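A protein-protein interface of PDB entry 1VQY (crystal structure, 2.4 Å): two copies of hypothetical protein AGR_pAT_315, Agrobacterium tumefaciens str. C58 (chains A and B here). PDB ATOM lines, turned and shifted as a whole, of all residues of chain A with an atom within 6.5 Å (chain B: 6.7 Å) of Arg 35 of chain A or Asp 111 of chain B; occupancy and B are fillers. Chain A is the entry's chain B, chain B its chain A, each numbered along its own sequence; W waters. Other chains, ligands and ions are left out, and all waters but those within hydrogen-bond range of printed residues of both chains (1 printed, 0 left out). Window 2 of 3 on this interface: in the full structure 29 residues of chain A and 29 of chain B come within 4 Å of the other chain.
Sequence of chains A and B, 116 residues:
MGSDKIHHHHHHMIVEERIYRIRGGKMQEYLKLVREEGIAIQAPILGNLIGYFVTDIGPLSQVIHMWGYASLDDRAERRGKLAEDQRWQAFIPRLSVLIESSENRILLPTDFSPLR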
ATOM      1  N   GLN A  28     -21.903 -11.921 -34.741  1.00  0.00           N
ATOM      2  CA  GLN A  28     -22.971 -11.769 -33.752  1.00  0.00           C
ATOM      3  C   GLN A  28     -24.084 -12.789 -33.943  1.00  0.00           C
ATOM      4  O   GLN A  28     -24.726 -13.194 -32.976  1.00  0.00           O
ATOM      5  CB  GLN A  28     -23.542 -10.349 -33.757  1.00  0.00           C
ATOM      6  CG  GLN A  28     -22.531  -9.270 -33.324  1.00  0.00           C
ATOM      7  CD  GLN A  28     -21.866  -9.564 -31.981  1.00  0.00           C
ATOM      8  OE1 GLN A  28     -22.543  -9.812 -30.978  1.00  0.00           O
ATOM      9  NE2 GLN A  28     -20.529  -9.559 -31.965  1.00  0.00           N
ATOM     10  N   TYR A  30     -23.532 -15.925 -35.303  1.00  0.00           N
ATOM     11  CA  TYR A  30     -22.861 -17.122 -34.782  1.00  0.00           C
ATOM     12  C   TYR A  30     -22.978 -17.191 -33.262  1.00  0.00           C
ATOM     13  O   TYR A  30     -23.446 -18.180 -32.716  1.00  0.00           O
ATOM     14  CB  TYR A  30     -21.371 -17.145 -35.161  1.00  0.00           C
ATOM     15  CG  TYR A  30     -20.664 -18.342 -34.596  1.00  0.00           C
ATOM     16  CD1 TYR A  30     -20.125 -18.309 -33.298  1.00  0.00           C
ATOM     17  CD2 TYR A  30     -20.550 -19.528 -35.327  1.00  0.00           C
ATOM     18  CE1 TYR A  30     -19.479 -19.413 -32.756  1.00  0.00           C
ATOM     19  CE2 TYR A  30     -19.908 -20.648 -34.785  1.00  0.00           C
ATOM     20  CZ  TYR A  30     -19.391 -20.581 -33.493  1.00  0.00           C
ATOM     21  OH  TYR A  30     -18.759 -21.667 -32.916  1.00  0.00           O
ATOM     22  N   LEU A  31     -22.536 -16.124 -32.601  1.00  0.00           N
ATOM     23  CA  LEU A  31     -22.571 -16.022 -31.156  1.00  0.00           C
ATOM     24  C   LEU A  31     -23.956 -16.169 -30.548  1.00  0.00           C
ATOM     25  O   LEU A  31     -24.116 -16.797 -29.495  1.00  0.00           O
ATOM     26  CB  LEU A  31     -21.976 -14.685 -30.728  1.00  0.00           C
ATOM     27  CG  LEU A  31     -20.459 -14.595 -30.829  1.00  0.00           C
ATOM     28  CD1 LEU A  31     -20.023 -13.203 -30.363  1.00  0.00           C
ATOM     29  CD2 LEU A  31     -19.742 -15.738 -30.033  1.00  0.00           C
ATOM     30  N   LYS A  32     -24.947 -15.576 -31.213  1.00  0.00           N
ATOM     31  CA  LYS A  32     -26.313 -15.561 -30.723  1.00  0.00           C
ATOM     32  C   LYS A  32     -26.902 -16.960 -30.752  1.00  0.00           C
ATOM     33  O   LYS A  32     -27.574 -17.377 -29.809  1.00  0.00           O
ATOM     34  CB  LYS A  32     -27.187 -14.613 -31.553  1.00  0.00           C
ATOM     35  CG  LYS A  32     -28.644 -14.614 -31.116  1.00  0.00           C
ATOM     36  CD  LYS A  32     -29.542 -13.735 -31.969  1.00  0.00           C
ATOM     37  CE  LYS A  32     -30.792 -13.355 -31.159  1.00  0.00           C
ATOM     38  NZ  LYS A  32     -31.776 -12.578 -31.944  1.00  0.00           N
ATOM     39  N   LEU A  33     -26.676 -17.665 -31.846  1.00  0.00           N
ATOM     40  CA  LEU A  33     -27.087 -19.062 -31.933  1.00  0.00           C
ATOM     41  C   LEU A  33     -26.491 -19.922 -30.822  1.00  0.00           C
ATOM     42  O   LEU A  33     -27.196 -20.721 -30.207  1.00  0.00           O
ATOM     43  CB  LEU A  33     -26.698 -19.652 -33.292  1.00  0.00           C
ATOM     44  CG  LEU A  33     -27.656 -19.249 -34.402  1.00  0.00           C
ATOM     45  CD1 LEU A  33     -27.012 -19.531 -35.741  1.00  0.00           C
ATOM     46  CD2 LEU A  33     -28.984 -19.979 -34.256  1.00  0.00           C
ATOM     47  N   VAL A  34     -25.205 -19.751 -30.553  1.00  0.00           N
ATOM     48  CA  VAL A  34     -24.559 -20.573 -29.553  1.00  0.00           C
ATOM     49  C   VAL A  34     -25.064 -20.165 -28.160  1.00  0.00           C
ATOM     50  O   VAL A  34     -25.517 -21.021 -27.390  1.00  0.00           O
ATOM     51  CB  VAL A  34     -23.012 -20.530 -29.677  1.00  0.00           C
ATOM     52  CG1 VAL A  34     -22.335 -21.356 -28.562  1.00  0.00           C
ATOM     53  CG2 VAL A  34     -22.588 -21.054 -31.051  1.00  0.00           C
ATOM     54  N   ARG A  35     -25.034 -18.867 -27.864  1.00  0.00           N
ATOM     55  CA  ARG A  35     -25.554 -18.330 -26.587  1.00  0.00           C
ATOM     56  C   ARG A  35     -26.951 -18.856 -26.247  1.00  0.00           C
ATOM     57  O   ARG A  35     -27.176 -19.425 -25.171  1.00  0.00           O
ATOM     58  CB  ARG A  35     -25.588 -16.794 -26.643  1.00  0.00           C
ATOM     59  CG  ARG A  35     -26.090 -16.112 -25.352  1.00  0.00           C
ATOM     60  CD  ARG A  35     -25.951 -14.589 -25.373  1.00  0.00           C
ATOM     61  NE  ARG A  35     -24.580 -14.195 -25.699  1.00  0.00           N
ATOM     62  CZ  ARG A  35     -24.172 -13.679 -26.862  1.00  0.00           C
ATOM     63  NH1 ARG A  35     -25.013 -13.436 -27.865  1.00  0.00           N
ATOM     64  NH2 ARG A  35     -22.899 -13.394 -27.026  1.00  0.00           N
ATOM     65  N   GLU A  36     -27.871 -18.676 -27.197  1.00  0.00           N
ATOM     66  CA  GLU A  36     -29.294 -18.902 -26.980  1.00  0.00           C
ATOM     67  C   GLU A  36     -29.773 -20.349 -27.144  1.00  0.00           C
ATOM     68  O   GLU A  36     -30.794 -20.719 -26.568  1.00  0.00           O
ATOM     69  CB  GLU A  36     -30.086 -18.000 -27.911  1.00  0.00           C
ATOM     70  CG  GLU A  36     -29.844 -16.503 -27.670  1.00  0.00           C
ATOM     71  CD  GLU A  36     -30.846 -15.616 -28.406  1.00  0.00           C
ATOM     72  OE1 GLU A  36     -31.637 -16.129 -29.225  1.00  0.00           O
ATOM     73  OE2 GLU A  36     -30.847 -14.393 -28.169  1.00  0.00           O
ATOM     74  N   GLU A  37     -29.047 -21.165 -27.910  1.00  0.00           N
ATOM     75  CA  GLU A  37     -29.455 -22.553 -28.167  1.00  0.00           C
ATOM     76  C   GLU A  37     -28.343 -23.589 -28.004  1.00  0.00           C
ATOM     77  O   GLU A  37     -28.498 -24.545 -27.251  1.00  0.00           O
ATOM     78  CB  GLU A  37     -30.033 -22.669 -29.576  1.00  0.00           C
ATOM     79  CG  GLU A  37     -31.327 -21.922 -29.731  1.00  0.00           C
ATOM     80  CD  GLU A  37     -31.837 -21.894 -31.157  1.00  0.00           C
ATOM     81  OE1 GLU A  37     -32.059 -22.989 -31.734  1.00  0.00           O
ATOM     82  OE2 GLU A  37     -32.032 -20.770 -31.679  1.00  0.00           O
ATOM     83  N   GLY A  38     -27.227 -23.395 -28.699  1.00  0.00           N
ATOM     84  CA  GLY A  38     -26.274 -24.470 -28.927  1.00  0.00           C
ATOM     85  C   GLY A  38     -25.515 -24.980 -27.725  1.00  0.00           C
ATOM     86  O   GLY A  38     -25.382 -26.184 -27.540  1.00  0.00           O
ATOM     87  N   ILE A  39     -25.040 -24.059 -26.897  1.00  0.00           N
ATOM     88  CA  ILE A  39     -24.222 -24.418 -25.746  1.00  0.00           C
ATOM     89  C   ILE A  39     -25.052 -25.152 -24.667  1.00  0.00           C
ATOM     90  O   ILE A  39     -24.525 -26.001 -23.931  1.00  0.00           O
ATOM     91  CB  ILE A  39     -23.459 -23.163 -25.195  1.00  0.00           C
ATOM     92  CG1 ILE A  39     -22.048 -23.533 -24.721  1.00  0.00           C
ATOM     93  CG2 ILE A  39     -24.269 -22.438 -24.067  1.00  0.00           C
ATOM     94  CD1 ILE A  39     -21.198 -24.240 -25.735  1.00  0.00           C
ATOM     95  N   ALA A  40     -26.353 -24.861 -24.612  1.00  0.00           N
ATOM     96  CA  ALA A  40     -27.274 -25.566 -23.713  1.00  0.00           C
ATOM     97  C   ALA A  40     -27.496 -27.042 -24.106  1.00  0.00           C
ATOM     98  O   ALA A  40     -27.789 -27.882 -23.247  1.00  0.00           O
ATOM     99  CB  ALA A  40     -28.620 -24.822 -23.619  1.00  0.00           C
ATOM    100  N   TYR A  52     -14.505 -20.317 -24.159  1.00  0.00           N
ATOM    101  CA  TYR A  52     -15.116 -19.988 -25.451  1.00  0.00           C
ATOM    102  C   TYR A  52     -14.773 -18.519 -25.757  1.00  0.00           C
ATOM    103  O   TYR A  52     -15.154 -17.622 -25.004  1.00  0.00           O
ATOM    104  CB  TYR A  52     -16.632 -20.226 -25.388  1.00  0.00           C
ATOM    105  CG  TYR A  52     -17.260 -20.698 -26.687  1.00  0.00           C
ATOM    106  CD1 TYR A  52     -17.211 -19.912 -27.846  1.00  0.00           C
ATOM    107  CD2 TYR A  52     -17.925 -21.924 -26.760  1.00  0.00           C
ATOM    108  CE1 TYR A  52     -17.796 -20.343 -29.027  1.00  0.00           C
ATOM    109  CE2 TYR A  52     -18.497 -22.365 -27.939  1.00  0.00           C
ATOM    110  CZ  TYR A  52     -18.441 -21.572 -29.072  1.00  0.00           C
ATOM    111  OH  TYR A  52     -19.040 -22.006 -30.248  1.00  0.00           O
ATOM    112  N   PRO B 109     -13.184 -13.664 -23.843  1.00  0.00           N
ATOM    113  CA  PRO B 109     -14.163 -14.697 -23.538  1.00  0.00           C
ATOM    114  C   PRO B 109     -15.577 -14.258 -23.807  1.00  0.00           C
ATOM    115  O   PRO B 109     -15.912 -13.104 -23.600  1.00  0.00           O
ATOM    116  CB  PRO B 109     -13.997 -14.903 -22.027  1.00  0.00           C
ATOM    117  CG  PRO B 109     -12.624 -14.437 -21.709  1.00  0.00           C
ATOM    118  CD  PRO B 109     -12.381 -13.303 -22.661  1.00  0.00           C
ATOM    119  N   THR B 110     -16.421 -15.179 -24.239  1.00  0.00           N
ATOM    120  CA  THR B 110     -17.823 -14.854 -24.419  1.00  0.00           C
ATOM    121  C   THR B 110     -18.514 -14.791 -23.049  1.00  0.00           C
ATOM    122  O   THR B 110     -17.935 -15.177 -22.036  1.00  0.00           O
ATOM    123  CB  THR B 110     -18.523 -15.851 -25.345  1.00  0.00           C
ATOM    124  OG1 THR B 110     -18.733 -17.090 -24.661  1.00  0.00           O
ATOM    125  CG2 THR B 110     -17.703 -16.077 -26.628  1.00  0.00           C
ATOM    126  N   ASP B 111     -19.741 -14.289 -23.007  1.00  0.00           N
ATOM    127  CA  ASP B 111     -20.495 -14.268 -21.748  1.00  0.00           C
ATOM    128  C   ASP B 111     -21.008 -15.662 -21.344  1.00  0.00           C
ATOM    129  O   ASP B 111     -21.660 -15.803 -20.312  1.00  0.00           O
ATOM    130  CB  ASP B 111     -21.640 -13.231 -21.779  1.00  0.00           C
ATOM    131  CG  ASP B 111     -22.709 -13.525 -22.823  1.00  0.00           C
ATOM    132  OD1 ASP B 111     -22.662 -14.550 -23.524  1.00  0.00           O
ATOM    133  OD2 ASP B 111     -23.624 -12.700 -22.936  1.00  0.00           O
ATOM    134  N   PHE B 112     -20.708 -16.677 -22.154  1.00  0.00           N
ATOM    135  CA  PHE B 112     -21.034 -18.062 -21.809  1.00  0.00           C
ATOM    136  C   PHE B 112     -19.800 -18.940 -21.702  1.00  0.00           C
ATOM    137  O   PHE B 112     -19.911 -20.145 -21.702  1.00  0.00           O
ATOM    138  CB  PHE B 112     -22.033 -18.662 -22.808  1.00  0.00           C
ATOM    139  CG  PHE B 112     -21.642 -18.512 -24.251  1.00  0.00           C
ATOM    140  CD1 PHE B 112     -20.788 -19.420 -24.853  1.00  0.00           C
ATOM    141  CD2 PHE B 112     -22.165 -17.475 -25.022  1.00  0.00           C
ATOM    142  CE1 PHE B 112     -20.443 -19.288 -26.198  1.00  0.00           C
ATOM    143  CE2 PHE B 112     -21.816 -17.334 -26.381  1.00  0.00           C
ATOM    144  CZ  PHE B 112     -20.971 -18.244 -26.961  1.00  0.00           C
ATOM    145  N   SER B 113     -18.629 -18.328 -21.589  1.00  0.00           N
ATOM    146  CA  SER B 113     -17.375 -19.042 -21.437  1.00  0.00           C
ATOM    147  C   SER B 113     -17.198 -19.303 -19.953  1.00  0.00           C
ATOM    148  O   SER B 113     -17.334 -18.383 -19.172  1.00  0.00           O
ATOM    149  CB  SER B 113     -16.219 -18.174 -21.970  1.00  0.00           C
ATOM    150  OG  SER B 113     -14.932 -18.754 -21.750  1.00  0.00           O
ATOM    151  N   PRO B 114     -16.931 -20.551 -19.553  1.00  0.00           N
ATOM    152  CA  PRO B 114     -16.556 -20.795 -18.151  1.00  0.00           C
ATOM    153  C   PRO B 114     -15.318 -20.022 -17.655  1.00  0.00           C
ATOM    154  O   PRO B 114     -15.239 -19.663 -16.475  1.00  0.00           O
ATOM    155  CB  PRO B 114     -16.336 -22.320 -18.098  1.00  0.00           C
ATOM    156  CG  PRO B 114     -17.206 -22.840 -19.198  1.00  0.00           C
ATOM    157  CD  PRO B 114     -17.043 -21.811 -20.298  1.00  0.00           C
ATOM    158  N   ARG B 116     -14.031 -16.639 -17.798  1.00  0.00           N
ATOM    159  CA  ARG B 116     -14.476 -15.297 -18.141  1.00  0.00           C
ATOM    160  C   ARG B 116     -14.432 -14.363 -16.931  1.00  0.00           C
ATOM    161  O   ARG B 116     -14.238 -14.808 -15.798  1.00  0.00           O
ATOM    162  CB  ARG B 116     -15.865 -15.336 -18.784  1.00  0.00           C
ATOM    163  CG  ARG B 116     -17.068 -15.374 -17.861  1.00  0.00           C
ATOM    164  CD  ARG B 116     -18.329 -15.174 -18.714  1.00  0.00           C
ATOM    165  NE  ARG B 116     -19.609 -15.310 -18.015  1.00  0.00           N
ATOM    166  CZ  ARG B 116     -20.156 -16.457 -17.610  1.00  0.00           C
ATOM    167  NH1 ARG B 116     -19.545 -17.617 -17.773  1.00  0.00           N
ATOM    168  NH2 ARG B 116     -21.327 -16.438 -17.016  1.00  0.00           N
ATOM    169  OXT ARG B 116     -14.549 -13.138 -17.040  1.00  0.00           O
HETATM  170  O   HOH W   1     -20.245 -12.820 -25.327  1.00  0.00           O
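The backbone NH (N) of Thr 110 of chain B lies within hydrogen-bond range of the backbone carbonyl oxygen (O) of Tyr 52 of chain A, at 2.9 Å. The side-chain hydroxyl (OG) of Ser 113 of chain B lies within hydrogen-bond range of the backbone NH (N) of Tyr 52 of chain A. OD1 of Asp 111 of chain B lies within salt-bridge range of NE of Arg 35 of chain A.
The side-chain hydroxyl of Tyr 30 of chain A sits at hydrogen-bond distance from the side-chain hydroxyl of Tyr 52 of chain A (2.7 Å). The backbone NH (N) of Phe 112 of chain B lies close to the side-chain hydroxyl (OG1) of Thr 110 of chain B, 3.2 Å away. The backbone NH (N) of Ser 113 of chain B sits at hydrogen-bond distance from the side-chain hydroxyl (OG1) of Thr 110 of chain B (3.3 Å). The backbone carbonyl oxygen (O) of Asp 111 of chain B lies within hydrogen-bond range of the guanidinium group (NE) of Arg 116 of chain B, 3.1 Å away. O of Ser 113 of chain B sits at hydrogen-bond distance from NH1 of Arg 116 of chain B, 2.7 Å away. The backbone carbonyl oxygen of Val 34 of chain A lies within hydrogen-bond range of the backbone NH of Ile 39 of chain A (3.1 Å).
CD2 of Leu 31 of chain A touches CG2 of Thr 110 of chain B, at 3.98 Å. O of Leu 31 of chain A touches CE2 of Phe 112 of chain B (3.9 Å). Val 34 of chain A touches Phe 112 of chain B (CG1 to CE1, 3.7 Å). CB of Arg 35 of chain A touches CE2 of Phe 112 of chain B (3.8 Å). O of Tyr 52 of chain A touches CA of Pro 109 of chain B (3.4 Å). Phe 112 of chain B touches Tyr 52 of chain A.
Arg 35 of chain A touches just these residues of chain B: Asp 111 and Phe 112. Asp 111 of chain B touches just one residue of chain A: Arg 35. Of the printed residues of chain A, Pro 109 of chain B touches Tyr 52. Of the printed residues of chain A, Phe 112 of chain B touches Leu 31, Val 34, Arg 35 and Tyr 52. Of the printed residues of chain B, Leu 31 of chain A touches Thr 110 (3.98 Å) and Phe 112 (3.9 Å). Leu 33 of chain A touches none of the printed residues of chain B. The nearest residue of chain B that does not touch Arg 35 of chain A is Thr 110 of chain B (5.3 Å). The nearest residue of chain A that does not touch Asp 111 of chain B is Tyr 52 of chain A (6.0 Å). The nearest printed residue of chain B that does not touch Leu 31 of chain A is Asp 111 of chain B (6.5 Å).
Printed residues of chain B that touch a printed residue of chain A: Pro 109, Thr 110, Asp 111, Phe 112 and Ser 113. Hydrophobic or aromatic side chains of chain B that line the printed part of chain A: Phe 112. Hydrophobic or aromatic side chains of chain A within 4 Å of the printed part of chain B: Leu 31, Val 34 and Tyr 52. Among the printed residues, 9 pairs touch across the chains. Among the printed residues, Asp or Glu carboxylates within 4 Å of a Lys or Arg side-chain nitrogen of the other chain: Arg 35 of chain A with Asp 111 of chain B.
No position is printed for both chains. Of the 9 pairs that touch across the chains among the printed residues, none has its exchanged pair printed and touching as well.
Water W1 bridges N of Asp 111 of chain B (2.8 Å) and NH2 of Arg 35 of chain A (3.2 Å).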
